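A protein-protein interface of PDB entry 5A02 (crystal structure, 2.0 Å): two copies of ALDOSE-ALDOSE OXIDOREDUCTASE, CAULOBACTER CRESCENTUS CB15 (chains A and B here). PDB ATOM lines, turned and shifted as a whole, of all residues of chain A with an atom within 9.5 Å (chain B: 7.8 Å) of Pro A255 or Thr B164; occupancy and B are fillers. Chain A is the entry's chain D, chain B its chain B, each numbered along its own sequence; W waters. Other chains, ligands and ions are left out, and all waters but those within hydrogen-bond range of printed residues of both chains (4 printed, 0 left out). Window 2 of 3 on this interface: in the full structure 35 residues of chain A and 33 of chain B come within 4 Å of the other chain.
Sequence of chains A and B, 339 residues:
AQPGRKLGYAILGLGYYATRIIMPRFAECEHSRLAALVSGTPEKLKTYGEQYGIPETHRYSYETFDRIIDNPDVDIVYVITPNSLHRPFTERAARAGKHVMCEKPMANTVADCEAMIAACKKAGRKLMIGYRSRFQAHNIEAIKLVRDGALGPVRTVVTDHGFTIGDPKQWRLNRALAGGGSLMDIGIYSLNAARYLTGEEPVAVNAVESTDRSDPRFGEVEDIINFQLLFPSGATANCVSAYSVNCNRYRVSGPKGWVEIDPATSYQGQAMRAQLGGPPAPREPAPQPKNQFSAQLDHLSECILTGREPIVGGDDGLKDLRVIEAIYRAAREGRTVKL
OD2 of Asp B223 lies within salt-bridge range of NH2 of Arg A155, at 2.7 Å. The side-chain hydroxyl of Ser B244 lies within hydrogen-bond range of the guanidinium group of Arg A155 (3.1 Å). O of Ser B244 lies close to N of Pro A255, at 3.5 Å.
N of Phe B163 lies within hydrogen-bond range of O of Val B245. The backbone NH (N) of Thr B164 lies within hydrogen-bond range of the side-chain amide oxygen (OD1) of Asn B246 (3.0 Å). OD1 of Asp B223 is in hydrogen-bond range of OG of Ser B244 (2.9 Å). N of Arg A155 lies within hydrogen-bond range of O of Ser A253, at 2.8 Å. The backbone carbonyl oxygen (O) of Thr A156 is in hydrogen-bond range of the backbone NH (N) of Ser A253 (2.9 Å). O of Trp A258 sits at hydrogen-bond distance from N of Gln A275, at 2.8 Å.
Val B245 touches Arg A155 (CG1 to CB, 3.5 Å). CB of Ser A253 touches CG1 of Val B245 (3.8 Å). Ser B244 touches Gly A254. CG1 of Val B245 touches O of Gly A254, 3.96 Å away. O of Pro A255 touches CG2 of Thr B164 (3.7 Å). Asn B246 touches Trp A258 (O to CD1, 3.5 Å).
Of chain B, only Ser B244 and Val B245 come within 4 Å of Gly A254. Printed residues of chain A within 4 Å of Asn B246: Trp A258 (3.5 Å). Printed residues of chain B within 4 Å of Arg A155: Asp B223 (2.7 Å), Ser B244 (3.1 Å) and Val B245 (3.5 Å).
Of the 17 printed residues of chain A, 5 touch a printed residue of chain B. Printed residues of chain B that touch a printed residue of chain A: Thr B164, Asp B223, Ser B244, Val B245 and Asn B246. Hydrophobic or aromatic side chains of chain B within 4 Å of the printed part of chain A: Val B245. Among the printed residues, Asp or Glu carboxylates within 4 Å of a Lys or Arg side-chain nitrogen of the other chain: Arg A155 with Asp B223 (2.7 Å).
No position is printed for both chains. Of the 9 pairs that touch across the chains among the printed residues, none has its exchanged pair printed and touching as well.
Water W1 lies within hydrogen-bond range of the side-chain amide oxygen of Gln A275 (2.6 Å) and the side-chain amide nitrogen of Asn B246 (2.9 Å). Water W4 bridges O of Gly A254 and N of Asn B246. Water W2 bridges the backbone carbonyl oxygen of Asn B246 and the side-chain hydroxyl of Ser A253. Water W3 bridges NE1 of Trp A258 (2.9 Å) and O of Asn B246 (3.4 Å).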
ATOM      1  N   GLY A 149      -2.246   7.649  10.401  1.00  0.00           N
ATOM      2  CA  GLY A 149      -2.015   8.562   9.295  1.00  0.00           C
ATOM      3  C   GLY A 149      -0.725   9.367   9.377  1.00  0.00           C
ATOM      4  O   GLY A 149      -0.526  10.302   8.605  1.00  0.00           O
ATOM      5  N   ALA A 150       0.148   9.007  10.311  1.00  0.00           N
ATOM      6  CA  ALA A 150       1.411   9.709  10.510  1.00  0.00           C
ATOM      7  C   ALA A 150       2.295   9.726   9.263  1.00  0.00           C
ATOM      8  O   ALA A 150       3.135  10.610   9.102  1.00  0.00           O
ATOM      9  CB  ALA A 150       2.172   9.078  11.666  1.00  0.00           C
ATOM     10  N   LEU A 151       2.118   8.751   8.382  1.00  0.00           N
ATOM     11  CA  LEU A 151       2.970   8.649   7.195  1.00  0.00           C
ATOM     12  C   LEU A 151       2.241   9.130   5.963  1.00  0.00           C
ATOM     13  O   LEU A 151       2.829   9.243   4.887  1.00  0.00           O
ATOM     14  CB  LEU A 151       3.429   7.203   6.954  1.00  0.00           C
ATOM     15  CG  LEU A 151       3.971   6.359   8.105  1.00  0.00           C
ATOM     16  CD1 LEU A 151       4.623   5.110   7.529  1.00  0.00           C
ATOM     17  CD2 LEU A 151       4.961   7.133   8.932  1.00  0.00           C
ATOM     18  N   GLY A 152       0.948   9.401   6.119  1.00  0.00           N
ATOM     19  CA  GLY A 152       0.088   9.592   4.970  1.00  0.00           C
ATOM     20  C   GLY A 152      -0.192   8.204   4.410  1.00  0.00           C
ATOM     21  O   GLY A 152       0.032   7.204   5.094  1.00  0.00           O
ATOM     22  N   PRO A 153      -0.687   8.134   3.171  1.00  0.00           N
ATOM     23  CA  PRO A 153      -0.942   6.848   2.517  1.00  0.00           C
ATOM     24  C   PRO A 153       0.344   6.043   2.369  1.00  0.00           C
ATOM     25  O   PRO A 153       1.367   6.585   1.940  1.00  0.00           O
ATOM     26  CB  PRO A 153      -1.499   7.248   1.154  1.00  0.00           C
ATOM     27  CG  PRO A 153      -1.001   8.647   0.928  1.00  0.00           C
ATOM     28  CD  PRO A 153      -0.955   9.280   2.284  1.00  0.00           C
ATOM     29  N   VAL A 154       0.307   4.767   2.728  1.00  0.00           N
ATOM     30  CA  VAL A 154       1.487   3.931   2.541  1.00  0.00           C
ATOM     31  C   VAL A 154       1.847   3.846   1.059  1.00  0.00           C
ATOM     32  O   VAL A 154       1.007   3.541   0.210  1.00  0.00           O
ATOM     33  CB  VAL A 154       1.278   2.529   3.116  1.00  0.00           C
ATOM     34  CG1 VAL A 154       2.457   1.623   2.760  1.00  0.00           C
ATOM     35  CG2 VAL A 154       1.118   2.627   4.632  1.00  0.00           C
ATOM     36  N   ARG A 155       3.101   4.140   0.750  1.00  0.00           N
ATOM     37  CA  ARG A 155       3.550   4.099  -0.625  1.00  0.00           C
ATOM     38  C   ARG A 155       4.495   2.933  -0.851  1.00  0.00           C
ATOM     39  O   ARG A 155       4.362   2.224  -1.841  1.00  0.00           O
ATOM     40  CB  ARG A 155       4.220   5.413  -1.015  1.00  0.00           C
ATOM     41  CG  ARG A 155       3.281   6.629  -0.915  1.00  0.00           C
ATOM     42  CD  ARG A 155       2.103   6.489  -1.877  1.00  0.00           C
ATOM     43  NE  ARG A 155       2.517   6.587  -3.276  1.00  0.00           N
ATOM     44  CZ  ARG A 155       1.970   5.894  -4.277  1.00  0.00           C
ATOM     45  NH1 ARG A 155       0.981   5.036  -4.048  1.00  0.00           N
ATOM     46  NH2 ARG A 155       2.402   6.068  -5.516  1.00  0.00           N
ATOM     47  N   THR A 156       5.452   2.740   0.054  1.00  0.00           N
ATOM     48  CA  THR A 156       6.379   1.625  -0.065  1.00  0.00           C
ATOM     49  C   THR A 156       6.574   0.883   1.256  1.00  0.00           C
ATOM     50  O   THR A 156       6.575   1.479   2.326  1.00  0.00           O
ATOM     51  CB  THR A 156       7.777   2.088  -0.567  1.00  0.00           C
ATOM     52  OG1 THR A 156       8.369   2.983   0.384  1.00  0.00           O
ATOM     53  CG2 THR A 156       7.685   2.782  -1.916  1.00  0.00           C
ATOM     54  N   VAL A 252       8.514   1.177   6.390  1.00  0.00           N
ATOM     55  CA  VAL A 252       7.286   1.544   5.694  1.00  0.00           C
ATOM     56  C   VAL A 252       7.288   3.064   5.508  1.00  0.00           C
ATOM     57  O   VAL A 252       7.594   3.798   6.441  1.00  0.00           O
ATOM     58  CB  VAL A 252       6.015   1.062   6.447  1.00  0.00           C
ATOM     59  CG1 VAL A 252       6.081   1.402   7.944  1.00  0.00           C
ATOM     60  CG2 VAL A 252       4.735   1.622   5.794  1.00  0.00           C
ATOM     61  N   SER A 253       6.986   3.521   4.291  1.00  0.00           N
ATOM     62  CA  SER A 253       7.088   4.943   3.955  1.00  0.00           C
ATOM     63  C   SER A 253       5.845   5.457   3.250  1.00  0.00           C
ATOM     64  O   SER A 253       5.192   4.741   2.478  1.00  0.00           O
ATOM     65  CB  SER A 253       8.304   5.224   3.056  1.00  0.00           C
ATOM     66  OG  SER A 253       9.464   4.563   3.526  1.00  0.00           O
ATOM     67  N   GLY A 254       5.532   6.716   3.525  1.00  0.00           N
ATOM     68  CA  GLY A 254       4.509   7.436   2.797  1.00  0.00           C
ATOM     69  C   GLY A 254       4.985   8.864   2.587  1.00  0.00           C
ATOM     70  O   GLY A 254       6.115   9.215   2.947  1.00  0.00           O
ATOM     71  N   PRO A 255       4.120   9.707   2.021  1.00  0.00           N
ATOM     72  CA  PRO A 255       4.591  11.048   1.660  1.00  0.00           C
ATOM     73  C   PRO A 255       4.905  11.916   2.877  1.00  0.00           C
ATOM     74  O   PRO A 255       5.672  12.854   2.732  1.00  0.00           O
ATOM     75  CB  PRO A 255       3.424  11.628   0.833  1.00  0.00           C
ATOM     76  CG  PRO A 255       2.234  10.811   1.191  1.00  0.00           C
ATOM     77  CD  PRO A 255       2.744   9.441   1.564  1.00  0.00           C
ATOM     78  N   LYS A 256       4.361  11.589   4.048  1.00  0.00           N
ATOM     79  CA  LYS A 256       4.602  12.401   5.245  1.00  0.00           C
ATOM     80  C   LYS A 256       5.808  11.938   6.060  1.00  0.00           C
ATOM     81  O   LYS A 256       6.265  12.637   6.966  1.00  0.00           O
ATOM     82  CB  LYS A 256       3.361  12.404   6.138  1.00  0.00           C
ATOM     83  CG  LYS A 256       2.159  13.161   5.570  1.00  0.00           C
ATOM     84  CD  LYS A 256       0.909  12.801   6.378  1.00  0.00           C
ATOM     85  CE  LYS A 256      -0.041  13.974   6.559  1.00  0.00           C
ATOM     86  NZ  LYS A 256      -0.713  14.373   5.294  1.00  0.00           N
ATOM     87  N   GLY A 257       6.332  10.759   5.754  1.00  0.00           N
ATOM     88  CA  GLY A 257       7.492  10.281   6.481  1.00  0.00           C
ATOM     89  C   GLY A 257       7.597   8.768   6.461  1.00  0.00           C
ATOM     90  O   GLY A 257       6.878   8.104   5.719  1.00  0.00           O
ATOM     91  N   TRP A 258       8.484   8.220   7.285  1.00  0.00           N
ATOM     92  CA  TRP A 258       8.641   6.779   7.334  1.00  0.00           C
ATOM     93  C   TRP A 258       9.057   6.292   8.712  1.00  0.00           C
ATOM     94  O   TRP A 258       9.524   7.059   9.550  1.00  0.00           O
ATOM     95  CB  TRP A 258       9.656   6.309   6.285  1.00  0.00           C
ATOM     96  CG  TRP A 258      11.014   6.995   6.292  1.00  0.00           C
ATOM     97  CD1 TRP A 258      11.434   7.995   5.448  1.00  0.00           C
ATOM     98  CD2 TRP A 258      12.135   6.691   7.136  1.00  0.00           C
ATOM     99  NE1 TRP A 258      12.736   8.336   5.732  1.00  0.00           N
ATOM    100  CE2 TRP A 258      13.192   7.551   6.756  1.00  0.00           C
ATOM    101  CE3 TRP A 258      12.348   5.781   8.181  1.00  0.00           C
ATOM    102  CZ2 TRP A 258      14.441   7.531   7.386  1.00  0.00           C
ATOM    103  CZ3 TRP A 258      13.589   5.763   8.805  1.00  0.00           C
ATOM    104  CH2 TRP A 258      14.617   6.636   8.404  1.00  0.00           C
ATOM    105  N   GLN A 275      11.420   8.946  10.527  1.00  0.00           N
ATOM    106  CA  GLN A 275      11.552  10.273   9.955  1.00  0.00           C
ATOM    107  C   GLN A 275      10.138  10.800   9.799  1.00  0.00           C
ATOM    108  O   GLN A 275       9.416  10.409   8.887  1.00  0.00           O
ATOM    109  CB  GLN A 275      12.317  10.231   8.624  1.00  0.00           C
ATOM    110  CG  GLN A 275      12.691  11.595   8.056  1.00  0.00           C
ATOM    111  CD  GLN A 275      11.539  12.245   7.329  1.00  0.00           C
ATOM    112  OE1 GLN A 275      11.177  11.824   6.233  1.00  0.00           O
ATOM    113  NE2 GLN A 275      10.932  13.263   7.946  1.00  0.00           N
ATOM    114  N   LEU A 276       9.715  11.647  10.729  1.00  0.00           N
ATOM    115  CA  LEU A 276       8.345  12.126  10.702  1.00  0.00           C
ATOM    116  C   LEU A 276       8.322  13.647  10.630  1.00  0.00           C
ATOM    117  O   LEU A 276       8.238  14.217   9.541  1.00  0.00           O
ATOM    118  CB  LEU A 276       7.586  11.608  11.927  1.00  0.00           C
ATOM    119  CG  LEU A 276       7.494  10.081  11.977  1.00  0.00           C
ATOM    120  CD1 LEU A 276       7.046   9.578  13.354  1.00  0.00           C
ATOM    121  CD2 LEU A 276       6.547   9.608  10.886  1.00  0.00           C
ATOM    122  N   GLY B 162      14.316   8.028  -3.742  1.00  0.00           N
ATOM    123  CA  GLY B 162      13.138   8.798  -4.074  1.00  0.00           C
ATOM    124  C   GLY B 162      13.094  10.099  -3.297  1.00  0.00           C
ATOM    125  O   GLY B 162      13.781  10.255  -2.289  1.00  0.00           O
ATOM    126  N   PHE B 163      12.286  11.040  -3.765  1.00  0.00           N
ATOM    127  CA  PHE B 163      11.998  12.215  -2.963  1.00  0.00           C
ATOM    128  C   PHE B 163      10.575  12.651  -3.251  1.00  0.00           C
ATOM    129  O   PHE B 163      10.017  12.332  -4.292  1.00  0.00           O
ATOM    130  CB  PHE B 163      13.011  13.341  -3.223  1.00  0.00           C
ATOM    131  CG  PHE B 163      12.958  13.913  -4.612  1.00  0.00           C
ATOM    132  CD1 PHE B 163      13.711  13.353  -5.634  1.00  0.00           C
ATOM    133  CD2 PHE B 163      12.184  15.033  -4.887  1.00  0.00           C
ATOM    134  CE1 PHE B 163      13.682  13.884  -6.915  1.00  0.00           C
ATOM    135  CE2 PHE B 163      12.140  15.572  -6.171  1.00  0.00           C
ATOM    136  CZ  PHE B 163      12.894  14.995  -7.188  1.00  0.00           C
ATOM    137  N   THR B 164       9.963  13.347  -2.305  1.00  0.00           N
ATOM    138  CA  THR B 164       8.602  13.802  -2.520  1.00  0.00           C
ATOM    139  C   THR B 164       8.629  15.058  -3.385  1.00  0.00           C
ATOM    140  O   THR B 164       9.007  16.144  -2.936  1.00  0.00           O
ATOM    141  CB  THR B 164       7.884  14.073  -1.192  1.00  0.00           C
ATOM    142  OG1 THR B 164       8.735  14.852  -0.351  1.00  0.00           O
ATOM    143  CG2 THR B 164       7.575  12.760  -0.479  1.00  0.00           C
ATOM    144  N   ILE B 165       8.230  14.903  -4.640  1.00  0.00           N
ATOM    145  CA  ILE B 165       8.335  15.998  -5.589  1.00  0.00           C
ATOM    146  C   ILE B 165       7.150  16.952  -5.409  1.00  0.00           C
ATOM    147  O   ILE B 165       6.092  16.559  -4.922  1.00  0.00           O
ATOM    148  CB  ILE B 165       8.419  15.449  -7.047  1.00  0.00           C
ATOM    149  CG1 ILE B 165       8.937  16.518  -8.020  1.00  0.00           C
ATOM    150  CG2 ILE B 165       7.079  14.846  -7.474  1.00  0.00           C
ATOM    151  CD1 ILE B 165       9.555  15.941  -9.338  1.00  0.00           C
ATOM    152  N   GLY B 166       7.331  18.213  -5.777  1.00  0.00           N
ATOM    153  CA  GLY B 166       6.286  19.201  -5.569  1.00  0.00           C
ATOM    154  C   GLY B 166       5.724  19.775  -6.853  1.00  0.00           C
ATOM    155  O   GLY B 166       5.009  19.096  -7.589  1.00  0.00           O
ATOM    156  N   ASP B 167       6.058  21.037  -7.096  1.00  0.00           N
ATOM    157  CA  ASP B 167       5.599  21.826  -8.244  1.00  0.00           C
ATOM    158  C   ASP B 167       5.315  21.043  -9.533  1.00  0.00           C
ATOM    159  O   ASP B 167       6.238  20.685 -10.259  1.00  0.00           O
ATOM    160  CB  ASP B 167       6.653  22.899  -8.519  1.00  0.00           C
ATOM    161  CG  ASP B 167       6.346  23.727  -9.736  1.00  0.00           C
ATOM    162  OD1 ASP B 167       5.159  23.806 -10.133  1.00  0.00           O
ATOM    163  OD2 ASP B 167       7.312  24.304 -10.284  1.00  0.00           O
ATOM    164  N   GLN B 170       7.044  21.824 -13.133  1.00  0.00           N
ATOM    165  CA  GLN B 170       8.484  21.735 -13.404  1.00  0.00           C
ATOM    166  C   GLN B 170       8.803  20.731 -14.518  1.00  0.00           C
ATOM    167  O   GLN B 170       7.981  19.863 -14.825  1.00  0.00           O
ATOM    168  CB  GLN B 170       9.225  21.351 -12.139  1.00  0.00           C
ATOM    169  CG  GLN B 170       8.917  19.947 -11.679  1.00  0.00           C
ATOM    170  CD  GLN B 170       9.589  19.651 -10.376  1.00  0.00           C
ATOM    171  OE1 GLN B 170      10.812  19.500 -10.323  1.00  0.00           O
ATOM    172  NE2 GLN B 170       8.808  19.602  -9.304  1.00  0.00           N
ATOM    173  N   ARG B 217       0.642  16.149 -10.283  1.00  0.00           N
ATOM    174  CA  ARG B 217       2.054  15.947 -10.596  1.00  0.00           C
ATOM    175  C   ARG B 217       2.290  14.856 -11.648  1.00  0.00           C
ATOM    176  O   ARG B 217       3.293  14.876 -12.359  1.00  0.00           O
ATOM    177  CB  ARG B 217       2.823  15.602  -9.313  1.00  0.00           C
ATOM    178  CG  ARG B 217       2.875  16.747  -8.293  1.00  0.00           C
ATOM    179  CD  ARG B 217       3.376  16.314  -6.912  1.00  0.00           C
ATOM    180  NE  ARG B 217       2.482  15.344  -6.279  1.00  0.00           N
ATOM    181  CZ  ARG B 217       2.804  14.596  -5.223  1.00  0.00           C
ATOM    182  NH1 ARG B 217       4.004  14.705  -4.663  1.00  0.00           N
ATOM    183  NH2 ARG B 217       1.922  13.731  -4.725  1.00  0.00           N
ATOM    184  N   PHE B 218       1.368  13.906 -11.754  1.00  0.00           N
ATOM    185  CA  PHE B 218       1.683  12.655 -12.439  1.00  0.00           C
ATOM    186  C   PHE B 218       0.799  12.306 -13.633  1.00  0.00           C
ATOM    187  O   PHE B 218       0.548  11.129 -13.902  1.00  0.00           O
ATOM    188  CB  PHE B 218       1.632  11.521 -11.423  1.00  0.00           C
ATOM    189  CG  PHE B 218       2.537  11.733 -10.240  1.00  0.00           C
ATOM    190  CD1 PHE B 218       3.874  12.070 -10.424  1.00  0.00           C
ATOM    191  CD2 PHE B 218       2.050  11.610  -8.947  1.00  0.00           C
ATOM    192  CE1 PHE B 218       4.706  12.270  -9.336  1.00  0.00           C
ATOM    193  CE2 PHE B 218       2.880  11.807  -7.851  1.00  0.00           C
ATOM    194  CZ  PHE B 218       4.204  12.137  -8.042  1.00  0.00           C
ATOM    195  N   ASP B 223       5.212   7.898 -10.909  1.00  0.00           N
ATOM    196  CA  ASP B 223       5.537   8.236  -9.544  1.00  0.00           C
ATOM    197  C   ASP B 223       6.446   7.137  -9.001  1.00  0.00           C
ATOM    198  O   ASP B 223       7.643   7.327  -8.873  1.00  0.00           O
ATOM    199  CB  ASP B 223       4.242   8.391  -8.731  1.00  0.00           C
ATOM    200  CG  ASP B 223       4.469   8.472  -7.222  1.00  0.00           C
ATOM    201  OD1 ASP B 223       5.620   8.613  -6.742  1.00  0.00           O
ATOM    202  OD2 ASP B 223       3.447   8.408  -6.505  1.00  0.00           O
ATOM    203  N   ALA B 242      10.989   6.400  -6.558  1.00  0.00           N
ATOM    204  CA  ALA B 242       9.746   7.061  -6.169  1.00  0.00           C
ATOM    205  C   ALA B 242       9.783   8.579  -6.221  1.00  0.00           C
ATOM    206  O   ALA B 242      10.819   9.207  -5.993  1.00  0.00           O
ATOM    207  CB  ALA B 242       9.346   6.622  -4.747  1.00  0.00           C
ATOM    208  N   TYR B 243       8.622   9.159  -6.487  1.00  0.00           N
ATOM    209  CA  TYR B 243       8.433  10.603  -6.383  1.00  0.00           C
ATOM    210  C   TYR B 243       7.463  10.959  -5.244  1.00  0.00           C
ATOM    211  O   TYR B 243       6.955  12.079  -5.188  1.00  0.00           O
ATOM    212  CB  TYR B 243       7.891  11.162  -7.700  1.00  0.00           C
ATOM    213  CG  TYR B 243       8.910  11.684  -8.693  1.00  0.00           C
ATOM    214  CD1 TYR B 243      10.207  12.034  -8.307  1.00  0.00           C
ATOM    215  CD2 TYR B 243       8.556  11.843 -10.031  1.00  0.00           C
ATOM    216  CE1 TYR B 243      11.126  12.535  -9.242  1.00  0.00           C
ATOM    217  CE2 TYR B 243       9.451  12.338 -10.960  1.00  0.00           C
ATOM    218  CZ  TYR B 243      10.732  12.683 -10.568  1.00  0.00           C
ATOM    219  OH  TYR B 243      11.592  13.178 -11.519  1.00  0.00           O
ATOM    220  N   SER B 244       7.183  10.014  -4.348  1.00  0.00           N
ATOM    221  CA  SER B 244       6.196  10.276  -3.297  1.00  0.00           C
ATOM    222  C   SER B 244       6.661   9.792  -1.927  1.00  0.00           C
ATOM    223  O   SER B 244       5.887   9.773  -0.975  1.00  0.00           O
ATOM    224  CB  SER B 244       4.860   9.629  -3.652  1.00  0.00           C
ATOM    225  OG  SER B 244       5.032   8.244  -3.926  1.00  0.00           O
ATOM    226  N   VAL B 245       7.920   9.377  -1.835  1.00  0.00           N
ATOM    227  CA  VAL B 245       8.552   9.092  -0.551  1.00  0.00           C
ATOM    228  C   VAL B 245       9.982   9.601  -0.615  1.00  0.00           C
ATOM    229  O   VAL B 245      10.564   9.701  -1.689  1.00  0.00           O
ATOM    230  CB  VAL B 245       8.579   7.575  -0.177  1.00  0.00           C
ATOM    231  CG1 VAL B 245       7.188   6.980  -0.137  1.00  0.00           C
ATOM    232  CG2 VAL B 245       9.468   6.794  -1.123  1.00  0.00           C
ATOM    233  N   ASN B 246      10.536   9.925   0.544  1.00  0.00           N
ATOM    234  CA  ASN B 246      11.927  10.321   0.657  1.00  0.00           C
ATOM    235  C   ASN B 246      12.783   9.156   1.127  1.00  0.00           C
ATOM    236  O   ASN B 246      12.591   8.636   2.217  1.00  0.00           O
ATOM    237  CB  ASN B 246      12.064  11.507   1.621  1.00  0.00           C
ATOM    238  CG  ASN B 246      11.434  12.756   1.068  1.00  0.00           C
ATOM    239  OD1 ASN B 246      11.877  13.275   0.045  1.00  0.00           O
ATOM    240  ND2 ASN B 246      10.379  13.233   1.713  1.00  0.00           N
ATOM    241  N   CYS B 247      13.730   8.748   0.291  1.00  0.00           N
ATOM    242  CA  CYS B 247      14.631   7.663   0.636  1.00  0.00           C
ATOM    243  C   CYS B 247      15.913   7.777  -0.176  1.00  0.00           C
ATOM    244  O   CYS B 247      15.902   8.229  -1.318  1.00  0.00           O
ATOM    245  CB  CYS B 247      13.963   6.294   0.399  1.00  0.00           C
ATOM    246  SG  CYS B 247      13.235   6.073  -1.267  1.00  0.00           S
HETATM  247  O   HOH W   1       9.477  12.219   4.247  1.00  0.00           O
HETATM  248  O   HOH W   2      11.990   5.929   2.795  1.00  0.00           O
HETATM  249  O   HOH W   3      14.050  10.659   4.525  1.00  0.00           O
HETATM  250  O   HOH W   4       8.893   9.717   2.987  1.00  0.00           O
